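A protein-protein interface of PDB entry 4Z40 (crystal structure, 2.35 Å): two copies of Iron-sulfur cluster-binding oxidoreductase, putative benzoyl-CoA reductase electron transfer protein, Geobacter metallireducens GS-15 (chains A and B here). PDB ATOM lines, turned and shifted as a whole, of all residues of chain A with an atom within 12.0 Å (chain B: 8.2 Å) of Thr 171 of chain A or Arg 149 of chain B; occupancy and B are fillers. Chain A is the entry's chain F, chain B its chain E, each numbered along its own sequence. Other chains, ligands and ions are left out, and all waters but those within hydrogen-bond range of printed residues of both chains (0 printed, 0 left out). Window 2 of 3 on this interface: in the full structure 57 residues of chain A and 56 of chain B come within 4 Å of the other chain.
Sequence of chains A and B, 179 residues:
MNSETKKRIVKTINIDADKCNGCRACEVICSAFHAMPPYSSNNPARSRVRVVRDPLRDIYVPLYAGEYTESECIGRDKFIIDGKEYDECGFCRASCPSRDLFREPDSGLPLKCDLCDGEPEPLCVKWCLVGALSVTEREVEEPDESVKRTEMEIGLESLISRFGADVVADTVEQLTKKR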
ATOM      1  N   ARG A 103       8.811  11.411  -5.000  1.00  0.00           N
ATOM      2  CA  ARG A 103       8.169  10.208  -5.512  1.00  0.00           C
ATOM      3  C   ARG A 103       6.896  10.575  -6.270  1.00  0.00           C
ATOM      4  O   ARG A 103       6.143  11.448  -5.830  1.00  0.00           O
ATOM      5  CB  ARG A 103       7.834   9.245  -4.381  1.00  0.00           C
ATOM      6  CG  ARG A 103       9.027   8.698  -3.656  1.00  0.00           C
ATOM      7  CD  ARG A 103       8.555   7.787  -2.555  1.00  0.00           C
ATOM      8  NE  ARG A 103       7.995   6.542  -3.068  1.00  0.00           N
ATOM      9  CZ  ARG A 103       7.203   5.740  -2.363  1.00  0.00           C
ATOM     10  NH1 ARG A 103       6.870   6.065  -1.123  1.00  0.00           N
ATOM     11  NH2 ARG A 103       6.738   4.619  -2.892  1.00  0.00           N
ATOM     12  N   PRO A 105       3.282  10.890  -7.338  1.00  0.00           N
ATOM     13  CA  PRO A 105       2.122  10.803  -6.444  1.00  0.00           C
ATOM     14  C   PRO A 105       1.120   9.724  -6.848  1.00  0.00           C
ATOM     15  O   PRO A 105       0.326   9.324  -5.996  1.00  0.00           O
ATOM     16  CB  PRO A 105       1.498  12.198  -6.541  1.00  0.00           C
ATOM     17  CG  PRO A 105       1.936  12.713  -7.864  1.00  0.00           C
ATOM     18  CD  PRO A 105       3.276  12.114  -8.158  1.00  0.00           C
ATOM     19  N   ASP A 106       1.162   9.250  -8.093  1.00  0.00           N
ATOM     20  CA  ASP A 106       0.245   8.199  -8.548  1.00  0.00           C
ATOM     21  C   ASP A 106       0.862   6.792  -8.573  1.00  0.00           C
ATOM     22  O   ASP A 106       0.145   5.792  -8.500  1.00  0.00           O
ATOM     23  CB  ASP A 106      -0.301   8.526  -9.952  1.00  0.00           C
ATOM     24  CG  ASP A 106       0.797   8.861 -10.952  1.00  0.00           C
ATOM     25  OD1 ASP A 106       1.996   8.759 -10.596  1.00  0.00           O
ATOM     26  OD2 ASP A 106       0.464   9.230 -12.103  1.00  0.00           O
ATOM     27  N   SER A 107       2.183   6.714  -8.693  1.00  0.00           N
ATOM     28  CA  SER A 107       2.868   5.433  -8.847  1.00  0.00           C
ATOM     29  C   SER A 107       3.868   5.156  -7.724  1.00  0.00           C
ATOM     30  O   SER A 107       4.034   4.018  -7.295  1.00  0.00           O
ATOM     31  CB  SER A 107       3.594   5.384 -10.190  1.00  0.00           C
ATOM     32  OG  SER A 107       4.673   6.307 -10.215  1.00  0.00           O
ATOM     33  N   GLY A 108       4.542   6.197  -7.261  1.00  0.00           N
ATOM     34  CA  GLY A 108       5.546   6.031  -6.228  1.00  0.00           C
ATOM     35  C   GLY A 108       6.945   5.913  -6.801  1.00  0.00           C
ATOM     36  O   GLY A 108       7.911   5.702  -6.069  1.00  0.00           O
ATOM     37  N   LEU A 109       7.050   6.048  -8.116  1.00  0.00           N
ATOM     38  CA  LEU A 109       8.332   5.975  -8.798  1.00  0.00           C
ATOM     39  C   LEU A 109       9.282   7.049  -8.299  1.00  0.00           C
ATOM     40  O   LEU A 109       8.863   8.176  -8.033  1.00  0.00           O
ATOM     41  CB  LEU A 109       8.152   6.117 -10.310  1.00  0.00           C
ATOM     42  CG  LEU A 109       7.672   4.886 -11.077  1.00  0.00           C
ATOM     43  CD1 LEU A 109       7.547   5.195 -12.578  1.00  0.00           C
ATOM     44  CD2 LEU A 109       8.603   3.700 -10.820  1.00  0.00           C
ATOM     45  N   LEU A 156      12.653   0.739 -12.952  1.00  0.00           N
ATOM     46  CA  LEU A 156      12.197  -0.640 -13.112  1.00  0.00           C
ATOM     47  C   LEU A 156      12.528  -1.476 -11.874  1.00  0.00           C
ATOM     48  O   LEU A 156      11.703  -2.260 -11.413  1.00  0.00           O
ATOM     49  CB  LEU A 156      12.815  -1.284 -14.365  1.00  0.00           C
ATOM     50  CG  LEU A 156      12.001  -1.494 -15.654  1.00  0.00           C
ATOM     51  CD1 LEU A 156      10.596  -2.016 -15.374  1.00  0.00           C
ATOM     52  CD2 LEU A 156      11.945  -0.237 -16.503  1.00  0.00           C
ATOM     53  N   SER A 158      13.083  -0.399  -8.749  1.00  0.00           N
ATOM     54  CA  SER A 158      12.262   0.030  -7.621  1.00  0.00           C
ATOM     55  C   SER A 158      10.883  -0.645  -7.651  1.00  0.00           C
ATOM     56  O   SER A 158      10.345  -1.008  -6.604  1.00  0.00           O
ATOM     57  CB  SER A 158      12.108   1.551  -7.609  1.00  0.00           C
ATOM     58  OG  SER A 158      11.394   2.005  -8.744  1.00  0.00           O
ATOM     59  N   LEU A 159      10.322  -0.820  -8.848  1.00  0.00           N
ATOM     60  CA  LEU A 159       9.054  -1.531  -9.008  1.00  0.00           C
ATOM     61  C   LEU A 159       9.207  -3.033  -8.761  1.00  0.00           C
ATOM     62  O   LEU A 159       8.344  -3.653  -8.141  1.00  0.00           O
ATOM     63  CB  LEU A 159       8.465  -1.292 -10.408  1.00  0.00           C
ATOM     64  CG  LEU A 159       7.709   0.015 -10.672  1.00  0.00           C
ATOM     65  CD1 LEU A 159       7.401   0.167 -12.150  1.00  0.00           C
ATOM     66  CD2 LEU A 159       6.424   0.078  -9.861  1.00  0.00           C
ATOM     67  N   ILE A 160      10.297  -3.616  -9.255  1.00  0.00           N
ATOM     68  CA  ILE A 160      10.557  -5.045  -9.069  1.00  0.00           C
ATOM     69  C   ILE A 160      10.784  -5.350  -7.589  1.00  0.00           C
ATOM     70  O   ILE A 160      10.411  -6.416  -7.094  1.00  0.00           O
ATOM     71  CB  ILE A 160      11.769  -5.515  -9.920  1.00  0.00           C
ATOM     72  CG1 ILE A 160      11.356  -5.602 -11.396  1.00  0.00           C
ATOM     73  CG2 ILE A 160      12.301  -6.857  -9.442  1.00  0.00           C
ATOM     74  CD1 ILE A 160      12.405  -6.202 -12.307  1.00  0.00           C
ATOM     75  N   SER A 161      11.361  -4.383  -6.882  1.00  0.00           N
ATOM     76  CA  SER A 161      11.587  -4.499  -5.446  1.00  0.00           C
ATOM     77  C   SER A 161      10.276  -4.409  -4.659  1.00  0.00           C
ATOM     78  O   SER A 161      10.148  -4.986  -3.579  1.00  0.00           O
ATOM     79  CB  SER A 161      12.558  -3.414  -4.978  1.00  0.00           C
ATOM     80  OG  SER A 161      12.684  -3.416  -3.568  1.00  0.00           O
ATOM     81  N   ARG A 162       9.304  -3.686  -5.210  1.00  0.00           N
ATOM     82  CA  ARG A 162       8.029  -3.465  -4.534  1.00  0.00           C
ATOM     83  C   ARG A 162       6.988  -4.537  -4.855  1.00  0.00           C
ATOM     84  O   ARG A 162       6.189  -4.909  -3.994  1.00  0.00           O
ATOM     85  CB  ARG A 162       7.462  -2.089  -4.902  1.00  0.00           C
ATOM     86  CG  ARG A 162       8.194  -0.904  -4.301  1.00  0.00           C
ATOM     87  CD  ARG A 162       7.765   0.394  -4.973  1.00  0.00           C
ATOM     88  NE  ARG A 162       6.382   0.756  -4.674  1.00  0.00           N
ATOM     89  CZ  ARG A 162       5.732   1.770  -5.239  1.00  0.00           C
ATOM     90  NH1 ARG A 162       6.334   2.529  -6.145  1.00  0.00           N
ATOM     91  NH2 ARG A 162       4.478   2.024  -4.897  1.00  0.00           N
ATOM     92  N   PHE A 163       6.997  -5.030  -6.091  1.00  0.00           N
ATOM     93  CA  PHE A 163       5.899  -5.867  -6.577  1.00  0.00           C
ATOM     94  C   PHE A 163       6.327  -7.264  -7.054  1.00  0.00           C
ATOM     95  O   PHE A 163       5.480  -8.123  -7.291  1.00  0.00           O
ATOM     96  CB  PHE A 163       5.150  -5.126  -7.695  1.00  0.00           C
ATOM     97  CG  PHE A 163       4.592  -3.793  -7.260  1.00  0.00           C
ATOM     98  CD1 PHE A 163       3.395  -3.718  -6.565  1.00  0.00           C
ATOM     99  CD2 PHE A 163       5.277  -2.616  -7.524  1.00  0.00           C
ATOM    100  CE1 PHE A 163       2.888  -2.497  -6.151  1.00  0.00           C
ATOM    101  CE2 PHE A 163       4.772  -1.392  -7.110  1.00  0.00           C
ATOM    102  CZ  PHE A 163       3.578  -1.335  -6.424  1.00  0.00           C
ATOM    103  N   GLY A 164       7.632  -7.497  -7.171  1.00  0.00           N
ATOM    104  CA  GLY A 164       8.137  -8.807  -7.553  1.00  0.00           C
ATOM    105  C   GLY A 164       8.480  -8.911  -9.027  1.00  0.00           C
ATOM    106  O   GLY A 164       7.767  -8.366  -9.874  1.00  0.00           O
ATOM    107  N   ALA A 165       9.563  -9.621  -9.337  1.00  0.00           N
ATOM    108  CA  ALA A 165      10.065  -9.705 -10.707  1.00  0.00           C
ATOM    109  C   ALA A 165       9.032 -10.280 -11.677  1.00  0.00           C
ATOM    110  O   ALA A 165       8.848  -9.754 -12.775  1.00  0.00           O
ATOM    111  CB  ALA A 165      11.340 -10.530 -10.751  1.00  0.00           C
ATOM    112  N   ASP A 166       8.351 -11.349 -11.266  1.00  0.00           N
ATOM    113  CA  ASP A 166       7.389 -12.028 -12.132  1.00  0.00           C
ATOM    114  C   ASP A 166       6.138 -11.186 -12.399  1.00  0.00           C
ATOM    115  O   ASP A 166       5.681 -11.096 -13.539  1.00  0.00           O
ATOM    116  CB  ASP A 166       7.002 -13.392 -11.538  1.00  0.00           C
ATOM    117  CG  ASP A 166       6.696 -13.328 -10.047  1.00  0.00           C
ATOM    118  OD1 ASP A 166       7.198 -12.411  -9.363  1.00  0.00           O
ATOM    119  OD2 ASP A 166       5.958 -14.209  -9.557  1.00  0.00           O
ATOM    120  N   VAL A 167       5.597 -10.563 -11.353  1.00  0.00           N
ATOM    121  CA  VAL A 167       4.421  -9.697 -11.473  1.00  0.00           C
ATOM    122  C   VAL A 167       4.667  -8.512 -12.416  1.00  0.00           C
ATOM    123  O   VAL A 167       3.795  -8.142 -13.201  1.00  0.00           O
ATOM    124  CB  VAL A 167       3.980  -9.158 -10.091  1.00  0.00           C
ATOM    125  CG1 VAL A 167       2.774  -8.241 -10.223  1.00  0.00           C
ATOM    126  CG2 VAL A 167       3.678 -10.308  -9.143  1.00  0.00           C
ATOM    127  N   VAL A 168       5.859  -7.924 -12.334  1.00  0.00           N
ATOM    128  CA  VAL A 168       6.217  -6.790 -13.183  1.00  0.00           C
ATOM    129  C   VAL A 168       6.473  -7.240 -14.628  1.00  0.00           C
ATOM    130  O   VAL A 168       6.059  -6.567 -15.573  1.00  0.00           O
ATOM    131  CB  VAL A 168       7.457  -6.046 -12.643  1.00  0.00           C
ATOM    132  CG1 VAL A 168       7.818  -4.881 -13.543  1.00  0.00           C
ATOM    133  CG2 VAL A 168       7.201  -5.551 -11.224  1.00  0.00           C
ATOM    134  N   ALA A 169       7.141  -8.380 -14.792  1.00  0.00           N
ATOM    135  CA  ALA A 169       7.449  -8.914 -16.120  1.00  0.00           C
ATOM    136  C   ALA A 169       6.185  -9.245 -16.895  1.00  0.00           C
ATOM    137  O   ALA A 169       6.095  -8.986 -18.095  1.00  0.00           O
ATOM    138  CB  ALA A 169       8.330 -10.152 -16.009  1.00  0.00           C
ATOM    139  N   ASP A 170       5.212  -9.817 -16.196  1.00  0.00           N
ATOM    140  CA  ASP A 170       3.958 -10.229 -16.814  1.00  0.00           C
ATOM    141  C   ASP A 170       3.106  -9.036 -17.218  1.00  0.00           C
ATOM    142  O   ASP A 170       2.534  -9.011 -18.308  1.00  0.00           O
ATOM    143  CB  ASP A 170       3.182 -11.137 -15.865  1.00  0.00           C
ATOM    144  CG  ASP A 170       3.793 -12.518 -15.765  1.00  0.00           C
ATOM    145  OD1 ASP A 170       4.098 -13.103 -16.830  1.00  0.00           O
ATOM    146  OD2 ASP A 170       3.976 -13.014 -14.631  1.00  0.00           O
ATOM    147  N   THR A 171       3.028  -8.046 -16.336  1.00  0.00           N
ATOM    148  CA  THR A 171       2.312  -6.813 -16.634  1.00  0.00           C
ATOM    149  C   THR A 171       2.888  -6.128 -17.872  1.00  0.00           C
ATOM    150  O   THR A 171       2.137  -5.667 -18.733  1.00  0.00           O
ATOM    151  CB  THR A 171       2.351  -5.837 -15.440  1.00  0.00           C
ATOM    152  OG1 THR A 171       1.712  -6.442 -14.308  1.00  0.00           O
ATOM    153  CG2 THR A 171       1.635  -4.540 -15.790  1.00  0.00           C
ATOM    154  N   VAL A 172       4.216  -6.078 -17.961  1.00  0.00           N
ATOM    155  CA  VAL A 172       4.902  -5.481 -19.108  1.00  0.00           C
ATOM    156  C   VAL A 172       4.542  -6.202 -20.413  1.00  0.00           C
ATOM    157  O   VAL A 172       4.410  -5.567 -21.464  1.00  0.00           O
ATOM    158  CB  VAL A 172       6.440  -5.486 -18.907  1.00  0.00           C
ATOM    159  CG1 VAL A 172       7.172  -5.140 -20.198  1.00  0.00           C
ATOM    160  CG2 VAL A 172       6.830  -4.510 -17.807  1.00  0.00           C
ATOM    161  N   GLU A 173       4.367  -7.519 -20.343  1.00  0.00           N
ATOM    162  CA  GLU A 173       3.962  -8.298 -21.513  1.00  0.00           C
ATOM    163  C   GLU A 173       2.547  -7.926 -21.966  1.00  0.00           C
ATOM    164  O   GLU A 173       2.274  -7.814 -23.161  1.00  0.00           O
ATOM    165  CB  GLU A 173       4.042  -9.799 -21.218  1.00  0.00           C
ATOM    166  N   GLN A 174       1.656  -7.722 -21.000  1.00  0.00           N
ATOM    167  CA  GLN A 174       0.269  -7.374 -21.289  1.00  0.00           C
ATOM    168  C   GLN A 174       0.082  -5.875 -21.546  1.00  0.00           C
ATOM    169  O   GLN A 174      -1.039  -5.373 -21.511  1.00  0.00           O
ATOM    170  CB  GLN A 174      -0.636  -7.820 -20.136  1.00  0.00           C
ATOM    171  N   LEU A 175       1.180  -5.168 -21.806  1.00  0.00           N
ATOM    172  CA  LEU A 175       1.130  -3.731 -22.072  1.00  0.00           C
ATOM    173  C   LEU A 175       1.915  -3.369 -23.330  1.00  0.00           C
ATOM    174  O   LEU A 175       1.936  -2.207 -23.744  1.00  0.00           O
ATOM    175  CB  LEU A 175       1.676  -2.935 -20.877  1.00  0.00           C
ATOM    176  CG  LEU A 175       0.811  -2.789 -19.619  1.00  0.00           C
ATOM    177  CD1 LEU A 175       1.570  -2.064 -18.516  1.00  0.00           C
ATOM    178  CD2 LEU A 175      -0.484  -2.059 -19.928  1.00  0.00           C
ATOM    179  N   THR A 176       2.562  -4.365 -23.930  1.00  0.00           N
ATOM    180  CA  THR A 176       3.421  -4.142 -25.092  1.00  0.00           C
ATOM    181  C   THR A 176       3.233  -5.210 -26.170  1.00  0.00           C
ATOM    182  O   THR A 176       2.323  -6.037 -26.092  1.00  0.00           O
ATOM    183  CB  THR A 176       4.915  -4.099 -24.682  1.00  0.00           C
ATOM    184  OG1 THR A 176       5.220  -5.230 -23.855  1.00  0.00           O
ATOM    185  CG2 THR A 176       5.232  -2.817 -23.915  1.00  0.00           C
ATOM    186  N   ASP B 144       0.224   0.233   3.209  1.00  0.00           N
ATOM    187  CA  ASP B 144      -0.919  -0.502   2.670  1.00  0.00           C
ATOM    188  C   ASP B 144      -0.583  -1.172   1.340  1.00  0.00           C
ATOM    189  O   ASP B 144      -1.470  -1.670   0.646  1.00  0.00           O
ATOM    190  CB  ASP B 144      -2.121   0.429   2.495  1.00  0.00           C
ATOM    191  N   LYS B 148      -2.873  -1.966  -3.688  1.00  0.00           N
ATOM    192  CA  LYS B 148      -1.825  -1.005  -4.019  1.00  0.00           C
ATOM    193  C   LYS B 148      -1.145  -1.363  -5.346  1.00  0.00           C
ATOM    194  O   LYS B 148      -0.169  -0.724  -5.742  1.00  0.00           O
ATOM    195  CB  LYS B 148      -0.793  -0.939  -2.886  1.00  0.00           C
ATOM    196  CG  LYS B 148       0.007   0.361  -2.812  1.00  0.00           C
ATOM    197  CD  LYS B 148       1.021   0.324  -1.674  1.00  0.00           C
ATOM    198  CE  LYS B 148       1.838   1.610  -1.600  1.00  0.00           C
ATOM    199  NZ  LYS B 148       2.829   1.598  -0.478  1.00  0.00           N
ATOM    200  N   ARG B 149      -1.668  -2.373  -6.038  1.00  0.00           N
ATOM    201  CA  ARG B 149      -1.031  -2.872  -7.259  1.00  0.00           C
ATOM    202  C   ARG B 149      -1.487  -2.132  -8.524  1.00  0.00           C
ATOM    203  O   ARG B 149      -1.092  -2.487  -9.635  1.00  0.00           O
ATOM    204  CB  ARG B 149      -1.286  -4.375  -7.417  1.00  0.00           C
ATOM    205  CG  ARG B 149      -0.195  -5.112  -8.183  1.00  0.00           C
ATOM    206  CD  ARG B 149      -0.593  -6.549  -8.478  1.00  0.00           C
ATOM    207  NE  ARG B 149      -0.498  -6.863  -9.904  1.00  0.00           N
ATOM    208  CZ  ARG B 149      -0.868  -8.022 -10.446  1.00  0.00           C
ATOM    209  NH1 ARG B 149      -1.364  -8.987  -9.683  1.00  0.00           N
ATOM    210  NH2 ARG B 149      -0.742  -8.217 -11.752  1.00  0.00           N
ATOM    211  N   THR B 150      -2.315  -1.105  -8.360  1.00  0.00           N
ATOM    212  CA  THR B 150      -2.640  -0.219  -9.474  1.00  0.00           C
ATOM    213  C   THR B 150      -1.563   0.847  -9.583  1.00  0.00           C
ATOM    214  O   THR B 150      -1.419   1.486 -10.624  1.00  0.00           O
ATOM    215  CB  THR B 150      -4.015   0.461  -9.316  1.00  0.00           C
ATOM    216  OG1 THR B 150      -4.020   1.275  -8.134  1.00  0.00           O
ATOM    217  CG2 THR B 150      -5.127  -0.581  -9.243  1.00  0.00           C
ATOM    218  N   GLU B 151      -0.819   1.040  -8.492  1.00  0.00           N
ATOM    219  CA  GLU B 151       0.337   1.930  -8.490  1.00  0.00           C
ATOM    220  C   GLU B 151       1.408   1.387  -9.426  1.00  0.00           C
ATOM    221  O   GLU B 151       2.055   2.145 -10.143  1.00  0.00           O
ATOM    222  CB  GLU B 151       0.912   2.097  -7.078  1.00  0.00           C
ATOM    223  CG  GLU B 151       0.267   3.192  -6.238  1.00  0.00           C
ATOM    224  CD  GLU B 151       1.079   3.525  -4.987  1.00  0.00           C
ATOM    225  OE1 GLU B 151       2.048   2.792  -4.692  1.00  0.00           O
ATOM    226  OE2 GLU B 151       0.756   4.521  -4.299  1.00  0.00           O
ATOM    227  N   MET B 152       1.586   0.067  -9.410  1.00  0.00           N
ATOM    228  CA  MET B 152       2.590  -0.589 -10.241  1.00  0.00           C
ATOM    229  C   MET B 152       2.345  -0.340 -11.722  1.00  0.00           C
ATOM    230  O   MET B 152       3.260   0.018 -12.465  1.00  0.00           O
ATOM    231  CB  MET B 152       2.612  -2.096  -9.978  1.00  0.00           C
ATOM    232  CG  MET B 152       3.559  -2.840 -10.901  1.00  0.00           C
ATOM    233  SD  MET B 152       3.006  -4.497 -11.320  1.00  0.00           S
ATOM    234  CE  MET B 152       1.351  -4.162 -11.915  1.00  0.00           C
ATOM    235  N   GLU B 153       1.096  -0.528 -12.137  1.00  0.00           N
ATOM    236  CA  GLU B 153       0.706  -0.423 -13.539  1.00  0.00           C
ATOM    237  C   GLU B 153       0.795   1.015 -14.061  1.00  0.00           C
ATOM    238  O   GLU B 153       1.184   1.247 -15.206  1.00  0.00           O
ATOM    239  CB  GLU B 153      -0.710  -0.972 -13.718  1.00  0.00           C
ATOM    240  CG  GLU B 153      -1.054  -1.358 -15.140  1.00  0.00           C
ATOM    241  CD  GLU B 153      -2.229  -2.315 -15.208  1.00  0.00           C
ATOM    242  OE1 GLU B 153      -2.650  -2.804 -14.136  1.00  0.00           O
ATOM    243  OE2 GLU B 153      -2.726  -2.576 -16.329  1.00  0.00           O
ATOM    244  N   ILE B 154       0.437   1.976 -13.214  1.00  0.00           N
ATOM    245  CA  ILE B 154       0.555   3.394 -13.551  1.00  0.00           C
ATOM    246  C   ILE B 154       2.019   3.803 -13.787  1.00  0.00           C
ATOM    247  O   ILE B 154       2.316   4.606 -14.677  1.00  0.00           O
ATOM    248  CB  ILE B 154      -0.074   4.275 -12.439  1.00  0.00           C
ATOM    249  CG1 ILE B 154      -1.600   4.255 -12.560  1.00  0.00           C
ATOM    250  CG2 ILE B 154       0.445   5.703 -12.498  1.00  0.00           C
ATOM    251  CD1 ILE B 154      -2.321   5.003 -11.471  1.00  0.00           C
ATOM    252  N   GLY B 155       2.932   3.230 -13.003  1.00  0.00           N
ATOM    253  CA  GLY B 155       4.347   3.532 -13.126  1.00  0.00           C
ATOM    254  C   GLY B 155       4.998   2.902 -14.342  1.00  0.00           C
ATOM    255  O   GLY B 155       5.885   3.488 -14.958  1.00  0.00           O
ATOM    256  N   LEU B 156       4.559   1.697 -14.684  1.00  0.00           N
ATOM    257  CA  LEU B 156       5.049   1.012 -15.874  1.00  0.00           C
ATOM    258  C   LEU B 156       4.607   1.727 -17.162  1.00  0.00           C
ATOM    259  O   LEU B 156       5.328   1.723 -18.159  1.00  0.00           O
ATOM    260  CB  LEU B 156       4.579  -0.444 -15.873  1.00  0.00           C
ATOM    261  CG  LEU B 156       5.258  -1.340 -14.836  1.00  0.00           C
ATOM    262  CD1 LEU B 156       4.569  -2.690 -14.750  1.00  0.00           C
ATOM    263  CD2 LEU B 156       6.732  -1.512 -15.168  1.00  0.00           C
ATOM    264  N   GLU B 157       3.434   2.353 -17.140  1.00  0.00           N
ATOM    265  CA  GLU B 157       2.984   3.141 -18.283  1.00  0.00           C
ATOM    266  C   GLU B 157       3.736   4.462 -18.388  1.00  0.00           C
ATOM    267  O   GLU B 157       3.938   4.988 -19.477  1.00  0.00           O
ATOM    268  CB  GLU B 157       1.484   3.407 -18.198  1.00  0.00           C
ATOM    269  CG  GLU B 157       0.631   2.205 -18.540  1.00  0.00           C
ATOM    270  CD  GLU B 157      -0.841   2.495 -18.383  1.00  0.00           C
ATOM    271  OE1 GLU B 157      -1.361   3.350 -19.136  1.00  0.00           O
ATOM    272  OE2 GLU B 157      -1.471   1.879 -17.495  1.00  0.00           O
ATOM    273  N   ILE B 160       7.011   3.662 -20.014  1.00  0.00           N
ATOM    274  CA  ILE B 160       6.807   3.390 -21.436  1.00  0.00           C
ATOM    275  C   ILE B 160       6.726   4.686 -22.256  1.00  0.00           C
ATOM    276  O   ILE B 160       7.301   4.778 -23.342  1.00  0.00           O
ATOM    277  CB  ILE B 160       5.534   2.539 -21.646  1.00  0.00           C
ATOM    278  CG1 ILE B 160       5.816   1.080 -21.283  1.00  0.00           C
ATOM    279  CG2 ILE B 160       5.034   2.634 -23.077  1.00  0.00           C
ATOM    280  CD1 ILE B 160       4.574   0.255 -21.078  1.00  0.00           C
ATOM    281  N   VAL B 172      13.258  -5.457 -18.914  1.00  0.00           N
ATOM    282  CA  VAL B 172      12.662  -6.375 -17.947  1.00  0.00           C
ATOM    283  C   VAL B 172      13.298  -7.766 -18.051  1.00  0.00           C
ATOM    284  O   VAL B 172      13.477  -8.460 -17.042  1.00  0.00           O
ATOM    285  CB  VAL B 172      11.132  -6.471 -18.147  1.00  0.00           C
ATOM    286  CG1 VAL B 172      10.556  -7.647 -17.386  1.00  0.00           C
ATOM    287  CG2 VAL B 172      10.460  -5.175 -17.715  1.00  0.00           C
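The side-chain carboxylate (OE1) of Glu 151 of chain B lies within salt-bridge range of the guanidinium group (NH2) of Arg 162 of chain A.
SD of Met 152 of chain B lies close to OG1 of Thr 171 of chain A.
The side-chain carboxylate (OE1) of Glu 151 of chain B sits close to the backbone carbonyl oxygen (O) of Ser 107 of chain A.
Gly 108 of chain A touches none of the printed residues of chain B.
Of the printed residues of chain B, Leu 159 of chain A touches Met 152 and Leu 156.
Of the printed residues of chain B, Ala 169 of chain A touches Val 172 (3.6 Å).
Of chain B, only Arg 149 (3.96 Å), Met 152 (3.3 Å) and Leu 156 (3.6 Å) come within 4 Å of Thr 171 of chain A.
Arg 149 of chain B touches just these residues of chain A: Val 167 (3.6 Å) and Thr 171 (3.96 Å).
Printed residues of chain A within 4 Å of Glu 151 of chain B: Asp 106, Ser 107 and Arg 162.
Met 152 of chain B touches just these residues of chain A: Leu 159 (3.9 Å), Phe 163 (3.7 Å), Val 167 (3.9 Å) and Thr 171 (3.3 Å).
No residue of chain A comes within 4 Å of Glu 153 of chain B.
Of the printed residues of chain A, Leu 156 of chain B touches Leu 156, Leu 159, Val 168, Thr 171 and Val 172.
The nearest residue of chain A that does not touch Arg 149 of chain B is Phe 163 of chain A (4.1 Å).
OG of Ser 107 of chain A is in hydrogen-bond range of N of Leu 109 of chain A (3.2 Å).
The backbone carbonyl oxygen of Ser 107 of chain A lies within hydrogen-bond range of the guanidinium group of Arg 162 of chain A (3.0 Å).
O of Val 167 of chain A sits at hydrogen-bond distance from OG1 of Thr 171 of chain A.
OG1 of Thr 176 of chain A sits at hydrogen-bond distance from O of Val 172 of chain A, 2.5 Å away.
Leu 156 of chain B touches its own counterpart, Leu 156 of chain A.
Leu 156 of chain A touches Val 172 of chain B, and with the chains exchanged Val 172 of chain A touches Leu 156 of chain B.
Val 172 of chain A touches its own counterpart, Val 172 of chain B.
Of the 22 pairs that touch across the chains among the printed residues, 4 have their exchanged pair printed and touching as well.
Asp 106 of chain A touches Ile 154 of chain B (CG to CG2, 3.5 Å).
Ser 107 of chain A touches Gly 155 of chain B (CB to CA, 3.6 Å).
Gly 155 of chain B touches Leu 109 of chain A (O to CD1, 3.4 Å).
Leu 156 of chain A touches Leu 156 of chain B (CD1 to CD2, 3.9 Å).
Met 152 of chain B touches Leu 159 of chain A.
Leu 156 of chain B touches Leu 159 of chain A (CD2 to CD1, 3.5 Å).
CG1 of Val 167 of chain A touches SD of Met 152 of chain B, 3.9 Å away.
Thr 171 of chain A touches Leu 156 of chain B.
Leu 156 of chain B touches Val 172 of chain A.
Val 172 of chain B touches Val 172 of chain A.
Of the 13 printed residues of chain B, 8 touch a printed residue of chain A.
Printed residues of chain B that touch a printed residue of chain A: Lys 148, Arg 149, Glu 151, Met 152, Ile 154, Gly 155, Leu 156 and Val 172.
Among the printed residues, Asp or Glu carboxylates within 4 Å of a Lys or Arg side-chain nitrogen of the other chain: Arg 162 of chain A with Glu 151 of chain B (2.6 Å).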
